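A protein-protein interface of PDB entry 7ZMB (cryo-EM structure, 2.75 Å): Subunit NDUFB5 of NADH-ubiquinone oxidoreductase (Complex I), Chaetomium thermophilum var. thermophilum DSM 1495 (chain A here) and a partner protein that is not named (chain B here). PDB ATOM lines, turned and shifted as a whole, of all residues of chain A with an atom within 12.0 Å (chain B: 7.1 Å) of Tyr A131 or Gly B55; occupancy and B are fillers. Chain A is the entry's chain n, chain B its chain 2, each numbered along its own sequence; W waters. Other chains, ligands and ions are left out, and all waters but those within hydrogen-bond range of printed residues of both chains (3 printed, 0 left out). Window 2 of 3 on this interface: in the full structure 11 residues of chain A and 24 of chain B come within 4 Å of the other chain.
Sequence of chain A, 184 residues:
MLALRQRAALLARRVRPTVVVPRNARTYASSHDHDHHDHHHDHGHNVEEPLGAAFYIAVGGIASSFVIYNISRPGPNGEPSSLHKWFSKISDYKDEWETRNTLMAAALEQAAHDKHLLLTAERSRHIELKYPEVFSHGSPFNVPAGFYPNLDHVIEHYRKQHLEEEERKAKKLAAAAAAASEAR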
ATOM      1  N   HIS A 126      13.205  -1.063  10.195  1.00  0.00           N
ATOM      2  CA  HIS A 126      14.526  -0.926  10.875  1.00  0.00           C
ATOM      3  C   HIS A 126      14.360  -0.614  12.370  1.00  0.00           C
ATOM      4  O   HIS A 126      13.705   0.396  12.681  1.00  0.00           O
ATOM      5  CB  HIS A 126      15.422   0.078  10.130  1.00  0.00           C
ATOM      6  CG  HIS A 126      16.583   0.605  10.906  1.00  0.00           C
ATOM      7  ND1 HIS A 126      17.566  -0.210  11.421  1.00  0.00           N
ATOM      8  CD2 HIS A 126      16.938   1.868  11.225  1.00  0.00           C
ATOM      9  CE1 HIS A 126      18.470   0.523  12.035  1.00  0.00           C
ATOM     10  NE2 HIS A 126      18.106   1.801  11.931  1.00  0.00           N
ATOM     11  N   ILE A 127      14.944  -1.440  13.255  1.00  0.00           N
ATOM     12  CA  ILE A 127      14.885  -1.170  14.716  1.00  0.00           C
ATOM     13  C   ILE A 127      16.167  -0.427  15.103  1.00  0.00           C
ATOM     14  O   ILE A 127      17.250  -0.931  14.809  1.00  0.00           O
ATOM     15  CB  ILE A 127      14.742  -2.504  15.477  1.00  0.00           C
ATOM     16  CG1 ILE A 127      13.567  -3.343  14.967  1.00  0.00           C
ATOM     17  CG2 ILE A 127      14.663  -2.272  16.978  1.00  0.00           C
ATOM     18  CD1 ILE A 127      12.220  -2.866  15.451  1.00  0.00           C
ATOM     19  N   GLU A 128      16.032   0.719  15.770  1.00  0.00           N
ATOM     20  CA  GLU A 128      17.201   1.496  16.262  1.00  0.00           C
ATOM     21  C   GLU A 128      17.196   1.301  17.769  1.00  0.00           C
ATOM     22  O   GLU A 128      16.136   1.518  18.358  1.00  0.00           O
ATOM     23  CB  GLU A 128      17.041   2.981  15.932  1.00  0.00           C
ATOM     24  CG  GLU A 128      18.342   3.678  15.596  1.00  0.00           C
ATOM     25  CD  GLU A 128      18.209   4.844  14.634  1.00  0.00           C
ATOM     26  OE1 GLU A 128      17.366   4.761  13.719  1.00  0.00           O
ATOM     27  OE2 GLU A 128      18.948   5.834  14.801  1.00  0.00           O
ATOM     28  N   LEU A 129      18.327   0.928  18.360  1.00  0.00           N
ATOM     29  CA  LEU A 129      18.329   0.580  19.801  1.00  0.00           C
ATOM     30  C   LEU A 129      17.980   1.761  20.706  1.00  0.00           C
ATOM     31  O   LEU A 129      18.629   2.812  20.570  1.00  0.00           O
ATOM     32  CB  LEU A 129      19.727   0.061  20.130  1.00  0.00           C
ATOM     33  CG  LEU A 129      20.223  -1.110  19.291  1.00  0.00           C
ATOM     34  CD1 LEU A 129      21.566  -1.599  19.806  1.00  0.00           C
ATOM     35  CD2 LEU A 129      19.213  -2.234  19.321  1.00  0.00           C
ATOM     36  N   LYS A 130      16.970   1.607  21.561  1.00  0.00           N
ATOM     37  CA  LYS A 130      16.662   2.612  22.608  1.00  0.00           C
ATOM     38  C   LYS A 130      17.885   2.717  23.498  1.00  0.00           C
ATOM     39  O   LYS A 130      18.176   3.811  23.984  1.00  0.00           O
ATOM     40  CB  LYS A 130      15.469   2.146  23.440  1.00  0.00           C
ATOM     41  CG  LYS A 130      14.113   2.181  22.755  1.00  0.00           C
ATOM     42  CD  LYS A 130      13.056   1.450  23.546  1.00  0.00           C
ATOM     43  CE  LYS A 130      11.650   1.779  23.103  1.00  0.00           C
ATOM     44  NZ  LYS A 130      10.672   0.802  23.629  1.00  0.00           N
ATOM     45  N   TYR A 131      18.536   1.582  23.719  1.00  0.00           N
ATOM     46  CA  TYR A 131      19.722   1.523  24.599  1.00  0.00           C
ATOM     47  C   TYR A 131      20.935   1.060  23.771  1.00  0.00           C
ATOM     48  O   TYR A 131      21.262  -0.127  23.845  1.00  0.00           O
ATOM     49  CB  TYR A 131      19.322   0.716  25.826  1.00  0.00           C
ATOM     50  CG  TYR A 131      20.353   0.533  26.902  1.00  0.00           C
ATOM     51  CD1 TYR A 131      20.783   1.601  27.666  1.00  0.00           C
ATOM     52  CD2 TYR A 131      20.841  -0.727  27.197  1.00  0.00           C
ATOM     53  CE1 TYR A 131      21.711   1.428  28.676  1.00  0.00           C
ATOM     54  CE2 TYR A 131      21.762  -0.917  28.206  1.00  0.00           C
ATOM     55  CZ  TYR A 131      22.198   0.166  28.943  1.00  0.00           C
ATOM     56  OH  TYR A 131      23.095  -0.015  29.947  1.00  0.00           O
ATOM     57  N   PRO A 132      21.620   1.916  22.967  1.00  0.00           N
ATOM     58  CA  PRO A 132      22.844   1.524  22.258  1.00  0.00           C
ATOM     59  C   PRO A 132      24.006   1.310  23.225  1.00  0.00           C
ATOM     60  O   PRO A 132      25.066   1.041  22.756  1.00  0.00           O
ATOM     61  CB  PRO A 132      23.233   2.780  21.461  1.00  0.00           C
ATOM     62  CG  PRO A 132      21.960   3.533  21.298  1.00  0.00           C
ATOM     63  CD  PRO A 132      21.302   3.327  22.639  1.00  0.00           C
ATOM     64  N   GLU A 133      23.763   1.420  24.531  1.00  0.00           N
ATOM     65  CA  GLU A 133      24.831   1.353  25.557  1.00  0.00           C
ATOM     66  C   GLU A 133      24.976  -0.106  25.975  1.00  0.00           C
ATOM     67  O   GLU A 133      25.832  -0.384  26.816  1.00  0.00           O
ATOM     68  CB  GLU A 133      24.403   2.239  26.729  1.00  0.00           C
ATOM     69  CG  GLU A 133      24.889   3.673  26.671  1.00  0.00           C
ATOM     70  CD  GLU A 133      23.984   4.667  25.975  1.00  0.00           C
ATOM     71  OE1 GLU A 133      23.001   4.233  25.360  1.00  0.00           O
ATOM     72  OE2 GLU A 133      24.268   5.874  26.062  1.00  0.00           O
ATOM     73  N   VAL A 134      24.141  -0.986  25.424  1.00  0.00           N
ATOM     74  CA  VAL A 134      24.251  -2.452  25.668  1.00  0.00           C
ATOM     75  C   VAL A 134      25.546  -2.902  25.000  1.00  0.00           C
ATOM     76  O   VAL A 134      25.996  -4.021  25.284  1.00  0.00           O
ATOM     77  CB  VAL A 134      23.037  -3.191  25.071  1.00  0.00           C
ATOM     78  CG1 VAL A 134      23.064  -3.221  23.550  1.00  0.00           C
ATOM     79  CG2 VAL A 134      22.842  -4.581  25.645  1.00  0.00           C
ATOM     80  N   PHE A 135      26.181  -2.042  24.203  1.00  0.00           N
ATOM     81  CA  PHE A 135      27.414  -2.423  23.471  1.00  0.00           C
ATOM     82  C   PHE A 135      28.587  -2.272  24.426  1.00  0.00           C
ATOM     83  O   PHE A 135      29.713  -2.616  24.049  1.00  0.00           O
ATOM     84  CB  PHE A 135      27.609  -1.571  22.218  1.00  0.00           C
ATOM     85  CG  PHE A 135      26.886  -2.012  20.973  1.00  0.00           C
ATOM     86  CD1 PHE A 135      27.256  -3.170  20.312  1.00  0.00           C
ATOM     87  CD2 PHE A 135      25.875  -1.238  20.432  1.00  0.00           C
ATOM     88  CE1 PHE A 135      26.610  -3.558  19.151  1.00  0.00           C
ATOM     89  CE2 PHE A 135      25.223  -1.632  19.274  1.00  0.00           C
ATOM     90  CZ  PHE A 135      25.598  -2.788  18.632  1.00  0.00           C
ATOM     91  N   SER A 136      28.314  -1.781  25.633  1.00  0.00           N
ATOM     92  CA  SER A 136      29.374  -1.535  26.643  1.00  0.00           C
ATOM     93  C   SER A 136      29.186  -2.502  27.810  1.00  0.00           C
ATOM     94  O   SER A 136      29.922  -2.379  28.803  1.00  0.00           O
ATOM     95  CB  SER A 136      29.314  -0.125  27.083  1.00  0.00           C
ATOM     96  OG  SER A 136      29.771   0.750  26.066  1.00  0.00           O
ATOM     97  N   HIS A 137      28.248  -3.441  27.666  1.00  0.00           N
ATOM     98  CA  HIS A 137      27.967  -4.464  28.705  1.00  0.00           C
ATOM     99  C   HIS A 137      29.017  -5.575  28.693  1.00  0.00           C
ATOM    100  O   HIS A 137      29.840  -5.615  27.760  1.00  0.00           O
ATOM    101  CB  HIS A 137      26.573  -5.068  28.491  1.00  0.00           C
ATOM    102  CG  HIS A 137      25.452  -4.212  28.965  1.00  0.00           C
ATOM    103  ND1 HIS A 137      24.231  -4.738  29.330  1.00  0.00           N
ATOM    104  CD2 HIS A 137      25.360  -2.879  29.145  1.00  0.00           C
ATOM    105  CE1 HIS A 137      23.431  -3.766  29.706  1.00  0.00           C
ATOM    106  NE2 HIS A 137      24.103  -2.619  29.604  1.00  0.00           N
ATOM    107  N   GLY A 138      28.978  -6.447  29.697  1.00  0.00           N
ATOM    108  CA  GLY A 138      29.941  -7.559  29.809  1.00  0.00           C
ATOM    109  C   GLY A 138      30.762  -7.468  31.071  1.00  0.00           C
ATOM    110  O   GLY A 138      31.146  -6.354  31.429  1.00  0.00           O
ATOM    111  N   SER A 139      31.054  -8.608  31.697  1.00  0.00           N
ATOM    112  CA  SER A 139      31.812  -8.630  32.976  1.00  0.00           C
ATOM    113  C   SER A 139      33.237  -8.117  32.780  1.00  0.00           C
ATOM    114  O   SER A 139      33.846  -8.455  31.764  1.00  0.00           O
ATOM    115  CB  SER A 139      31.815 -10.008  33.569  1.00  0.00           C
ATOM    116  OG  SER A 139      32.412 -10.004  34.853  1.00  0.00           O
ATOM    117  N   LEU A 151      34.490  -3.885  18.511  1.00  0.00           N
ATOM    118  CA  LEU A 151      33.307  -3.132  18.002  1.00  0.00           C
ATOM    119  C   LEU A 151      33.671  -1.677  17.686  1.00  0.00           C
ATOM    120  O   LEU A 151      32.856  -0.805  18.000  1.00  0.00           O
ATOM    121  CB  LEU A 151      32.191  -3.189  19.050  1.00  0.00           C
ATOM    122  CG  LEU A 151      31.843  -4.571  19.599  1.00  0.00           C
ATOM    123  CD1 LEU A 151      30.990  -4.442  20.848  1.00  0.00           C
ATOM    124  CD2 LEU A 151      31.130  -5.408  18.551  1.00  0.00           C
ATOM    125  N   VAL A 154      31.078   0.043  15.284  1.00  0.00           N
ATOM    126  CA  VAL A 154      29.813   0.466  15.955  1.00  0.00           C
ATOM    127  C   VAL A 154      30.037   1.841  16.595  1.00  0.00           C
ATOM    128  O   VAL A 154      29.155   2.696  16.474  1.00  0.00           O
ATOM    129  CB  VAL A 154      29.352  -0.571  16.998  1.00  0.00           C
ATOM    130  CG1 VAL A 154      27.914  -0.344  17.407  1.00  0.00           C
ATOM    131  CG2 VAL A 154      29.547  -1.989  16.497  1.00  0.00           C
ATOM    132  N   ILE A 155      31.188   2.031  17.238  1.00  0.00           N
ATOM    133  CA  ILE A 155      31.486   3.321  17.916  1.00  0.00           C
ATOM    134  C   ILE A 155      31.575   4.409  16.845  1.00  0.00           C
ATOM    135  O   ILE A 155      31.091   5.518  17.099  1.00  0.00           O
ATOM    136  CB  ILE A 155      32.738   3.226  18.819  1.00  0.00           C
ATOM    137  CG1 ILE A 155      32.807   1.902  19.582  1.00  0.00           C
ATOM    138  CG2 ILE A 155      32.806   4.409  19.767  1.00  0.00           C
ATOM    139  CD1 ILE A 155      31.680   1.692  20.556  1.00  0.00           C
ATOM    140  N   HIS A 157      29.973   4.484  13.987  1.00  0.00           N
ATOM    141  CA  HIS A 157      28.588   4.753  13.547  1.00  0.00           C
ATOM    142  C   HIS A 157      27.887   5.665  14.555  1.00  0.00           C
ATOM    143  O   HIS A 157      27.240   6.633  14.128  1.00  0.00           O
ATOM    144  CB  HIS A 157      27.897   3.398  13.402  1.00  0.00           C
ATOM    145  CG  HIS A 157      26.409   3.423  13.405  1.00  0.00           C
ATOM    146  ND1 HIS A 157      25.674   3.318  12.246  1.00  0.00           N
ATOM    147  CD2 HIS A 157      25.517   3.499  14.414  1.00  0.00           C
ATOM    148  CE1 HIS A 157      24.394   3.353  12.538  1.00  0.00           C
ATOM    149  NE2 HIS A 157      24.273   3.465  13.860  1.00  0.00           N
ATOM    150  N   TYR A 158      28.018   5.361  15.842  1.00  0.00           N
ATOM    151  CA  TYR A 158      27.351   6.167  16.896  1.00  0.00           C
ATOM    152  C   TYR A 158      27.960   7.568  16.955  1.00  0.00           C
ATOM    153  O   TYR A 158      27.212   8.530  17.174  1.00  0.00           O
ATOM    154  CB  TYR A 158      27.222   5.387  18.204  1.00  0.00           C
ATOM    155  CG  TYR A 158      26.156   4.324  18.173  1.00  0.00           C
ATOM    156  CD1 TYR A 158      24.833   4.653  17.935  1.00  0.00           C
ATOM    157  CD2 TYR A 158      26.467   2.992  18.375  1.00  0.00           C
ATOM    158  CE1 TYR A 158      23.846   3.683  17.895  1.00  0.00           C
ATOM    159  CE2 TYR A 158      25.492   2.011  18.349  1.00  0.00           C
ATOM    160  CZ  TYR A 158      24.177   2.358  18.106  1.00  0.00           C
ATOM    161  OH  TYR A 158      23.211   1.398  18.087  1.00  0.00           O
ATOM    162  N   GLN A 161      26.385   9.565  14.145  1.00  0.00           N
ATOM    163  CA  GLN A 161      25.000   9.982  14.474  1.00  0.00           C
ATOM    164  C   GLN A 161      25.057  11.201  15.401  1.00  0.00           C
ATOM    165  O   GLN A 161      24.330  12.167  15.117  1.00  0.00           O
ATOM    166  CB  GLN A 161      24.203   8.799  15.027  1.00  0.00           C
ATOM    167  CG  GLN A 161      22.711   9.052  15.157  1.00  0.00           C
ATOM    168  CD  GLN A 161      22.014   7.897  15.833  1.00  0.00           C
ATOM    169  OE1 GLN A 161      20.818   7.944  16.111  1.00  0.00           O
ATOM    170  NE2 GLN A 161      22.764   6.843  16.106  1.00  0.00           N
ATOM    171  N   GLY B  50      12.171   5.788  21.333  1.00  0.00           N
ATOM    172  CA  GLY B  50      12.409   5.381  22.727  1.00  0.00           C
ATOM    173  C   GLY B  50      13.815   5.660  23.215  1.00  0.00           C
ATOM    174  O   GLY B  50      14.748   5.523  22.421  1.00  0.00           O
ATOM    175  N   ILE B  51      13.963   5.979  24.497  1.00  0.00           N
ATOM    176  CA  ILE B  51      15.303   6.195  25.104  1.00  0.00           C
ATOM    177  C   ILE B  51      15.455   5.235  26.278  1.00  0.00           C
ATOM    178  O   ILE B  51      14.694   5.381  27.237  1.00  0.00           O
ATOM    179  CB  ILE B  51      15.475   7.659  25.546  1.00  0.00           C
ATOM    180  CG1 ILE B  51      15.396   8.639  24.374  1.00  0.00           C
ATOM    181  CG2 ILE B  51      16.741   7.856  26.362  1.00  0.00           C
ATOM    182  CD1 ILE B  51      15.234  10.070  24.812  1.00  0.00           C
ATOM    183  N   GLY B  52      16.382   4.278  26.185  1.00  0.00           N
ATOM    184  CA  GLY B  52      16.675   3.354  27.260  1.00  0.00           C
ATOM    185  C   GLY B  52      17.138   4.050  28.522  1.00  0.00           C
ATOM    186  O   GLY B  52      18.016   4.912  28.475  1.00  0.00           O
ATOM    187  N   LEU B  53      16.558   3.683  29.656  1.00  0.00           N
ATOM    188  CA  LEU B  53      16.927   4.317  30.944  1.00  0.00           C
ATOM    189  C   LEU B  53      17.392   3.269  31.937  1.00  0.00           C
ATOM    190  O   LEU B  53      17.079   2.097  31.727  1.00  0.00           O
ATOM    191  CB  LEU B  53      15.713   5.047  31.528  1.00  0.00           C
ATOM    192  CG  LEU B  53      15.215   6.278  30.775  1.00  0.00           C
ATOM    193  CD1 LEU B  53      14.108   6.948  31.568  1.00  0.00           C
ATOM    194  CD2 LEU B  53      16.343   7.262  30.522  1.00  0.00           C
ATOM    195  N   HIS B  54      18.162   3.681  32.939  1.00  0.00           N
ATOM    196  CA  HIS B  54      18.542   2.791  34.067  1.00  0.00           C
ATOM    197  C   HIS B  54      19.140   1.456  33.622  1.00  0.00           C
ATOM    198  O   HIS B  54      18.594   0.413  34.009  1.00  0.00           O
ATOM    199  CB  HIS B  54      17.365   2.662  35.037  1.00  0.00           C
ATOM    200  CG  HIS B  54      16.914   3.951  35.635  1.00  0.00           C
ATOM    201  ND1 HIS B  54      17.554   4.527  36.710  1.00  0.00           N
ATOM    202  CD2 HIS B  54      15.885   4.767  35.325  1.00  0.00           C
ATOM    203  CE1 HIS B  54      16.946   5.647  37.033  1.00  0.00           C
ATOM    204  NE2 HIS B  54      15.920   5.818  36.196  1.00  0.00           N
ATOM    205  N   GLY B  55      20.201   1.482  32.820  1.00  0.00           N
ATOM    206  CA  GLY B  55      20.854   0.222  32.432  1.00  0.00           C
ATOM    207  C   GLY B  55      20.062  -0.600  31.449  1.00  0.00           C
ATOM    208  O   GLY B  55      20.268  -1.798  31.442  1.00  0.00           O
ATOM    209  N   GLY B  56      19.181   0.026  30.666  1.00  0.00           N
ATOM    210  CA  GLY B  56      18.382  -0.670  29.640  1.00  0.00           C
ATOM    211  C   GLY B  56      17.092  -1.247  30.181  1.00  0.00           C
ATOM    212  O   GLY B  56      16.239  -1.617  29.369  1.00  0.00           O
ATOM    213  N   LEU B  57      16.943  -1.316  31.498  1.00  0.00           N
ATOM    214  CA  LEU B  57      15.766  -1.953  32.136  1.00  0.00           C
ATOM    215  C   LEU B  57      14.472  -1.185  31.860  1.00  0.00           C
ATOM    216  O   LEU B  57      13.411  -1.823  31.758  1.00  0.00           O
ATOM    217  CB  LEU B  57      16.069  -2.137  33.624  1.00  0.00           C
ATOM    218  CG  LEU B  57      17.249  -3.069  33.906  1.00  0.00           C
ATOM    219  CD1 LEU B  57      17.296  -3.481  35.368  1.00  0.00           C
ATOM    220  CD2 LEU B  57      17.190  -4.299  33.014  1.00  0.00           C
ATOM    221  N   LEU B  58      14.555   0.136  31.783  1.00  0.00           N
ATOM    222  CA  LEU B  58      13.349   0.970  31.570  1.00  0.00           C
ATOM    223  C   LEU B  58      13.538   1.799  30.299  1.00  0.00           C
ATOM    224  O   LEU B  58      14.657   1.832  29.803  1.00  0.00           O
ATOM    225  CB  LEU B  58      13.127   1.848  32.808  1.00  0.00           C
ATOM    226  CG  LEU B  58      12.874   1.114  34.121  1.00  0.00           C
ATOM    227  CD1 LEU B  58      13.018   2.063  35.296  1.00  0.00           C
ATOM    228  CD2 LEU B  58      11.502   0.458  34.125  1.00  0.00           C
ATOM    229  N   ASN B 143      11.234  -2.307  29.682  1.00  0.00           N
ATOM    230  CA  ASN B 143      11.980  -2.599  28.432  1.00  0.00           C
ATOM    231  C   ASN B 143      12.566  -4.010  28.511  1.00  0.00           C
ATOM    232  O   ASN B 143      13.161  -4.462  27.529  1.00  0.00           O
ATOM    233  CB  ASN B 143      13.069  -1.539  28.228  1.00  0.00           C
ATOM    234  CG  ASN B 143      13.666  -1.517  26.838  1.00  0.00           C
ATOM    235  OD1 ASN B 143      12.948  -1.608  25.845  1.00  0.00           O
ATOM    236  ND2 ASN B 143      14.980  -1.388  26.763  1.00  0.00           N
ATOM    237  N   ASP B 144      12.436  -4.662  29.660  1.00  0.00           N
ATOM    238  CA  ASP B 144      13.028  -6.008  29.863  1.00  0.00           C
ATOM    239  C   ASP B 144      11.919  -7.023  30.158  1.00  0.00           C
ATOM    240  O   ASP B 144      10.845  -6.585  30.594  1.00  0.00           O
ATOM    241  CB  ASP B 144      14.009  -5.901  31.024  1.00  0.00           C
ATOM    242  CG  ASP B 144      14.953  -7.069  31.156  1.00  0.00           C
ATOM    243  OD1 ASP B 144      14.584  -8.019  31.857  1.00  0.00           O
ATOM    244  OD2 ASP B 144      16.049  -6.998  30.573  1.00  0.00           O
ATOM    245  N   ASP B 207      14.340  -5.186  23.460  1.00  0.00           N
ATOM    246  CA  ASP B 207      15.036  -4.592  22.331  1.00  0.00           C
ATOM    247  C   ASP B 207      15.814  -5.657  21.560  1.00  0.00           C
ATOM    248  O   ASP B 207      15.853  -5.640  20.325  1.00  0.00           O
ATOM    249  CB  ASP B 207      15.942  -3.483  22.861  1.00  0.00           C
ATOM    250  CG  ASP B 207      16.554  -2.638  21.777  1.00  0.00           C
ATOM    251  OD1 ASP B 207      16.315  -2.912  20.587  1.00  0.00           O
ATOM    252  OD2 ASP B 207      17.273  -1.678  22.124  1.00  0.00           O
HETATM  253  O   HOH W   1      15.108  -0.209  20.757  1.00  0.00           O
HETATM  254  O   HOH W   2      12.143  -1.706  22.537  1.00  0.00           O
HETATM  255  O   HOH W   3      19.714  -2.457  23.482  1.00  0.00           O
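The backbone NH (N) of Gly B52 lies within hydrogen-bond range of the backbone carbonyl oxygen (O) of Lys A130 (2.9 Å).
OD2 of Asp B207 lies within hydrogen-bond range of N of Lys A130 (3.3 Å).
Water W1 lies within hydrogen-bond range of N of Lys A130 (2.7 Å), OD2 of Asp B207 (3.0 Å) and O of Glu A128 (3.1 Å).
Water W3 bridges the backbone carbonyl oxygen of Tyr A131 (2.8 Å) and the side-chain carboxylate of Asp B207 (2.9 Å).
Water W2 lies within hydrogen-bond range of NZ of Lys A130 (3.1 Å) and OD1 of Asn B143 (3.4 Å).
CD2 of Leu A129 touches OD1 of Asp B207, 3.2 Å away.
Lys A130 touches Gly B50.
Lys A130 touches Ile B51 (O to C, 3.8 Å).
CD of Lys A130 touches OD1 of Asn B143 (3.8 Å).
Gly B55 touches Tyr A131 (CA to OH, 3.4 Å).
CD2 of Tyr A131 touches CA of Gly B56 (3.5 Å).
Tyr A131 touches Asp B207.
Printed residues of chain B within 4 Å of Leu A129: Asp B207.
Of the printed residues of chain B, Tyr A131 touches Gly B55, Gly B56 and Asp B207.
Printed residues of chain A within 4 Å of Gly B50: Lys A130.
His B54 touches none of the printed residues of chain A.
Gly B55 touches just one residue of chain A: Tyr A131 (3.4 Å).
Of chain A, only Tyr A131 (3.5 Å) comes within 4 Å of Gly B56.
Of the printed residues of chain A, Asp B207 touches Leu A129, Lys A130 and Tyr A131.
The nearest printed residue of chain B that does not touch Tyr A131 is Gly B52 (4.003 Å).
ND2 of Asn B143 sits at hydrogen-bond distance from O of Gly B56.
N of Asn B143 sits at hydrogen-bond distance from O of Leu B57 (3.0 Å).
OH of Tyr A131 lies within hydrogen-bond range of NE2 of His A137, at 2.8 Å.
Of the 20 printed residues of chain A, 3 touch a printed residue of chain B.
Hydrophobic or aromatic side chains of chain A within 4 Å of the printed part of chain B: Leu A129 and Tyr A131.
Among the printed residues, no Asp or Glu carboxylate lies within 4 Å of a Lys or Arg side-chain nitrogen of the other chain.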
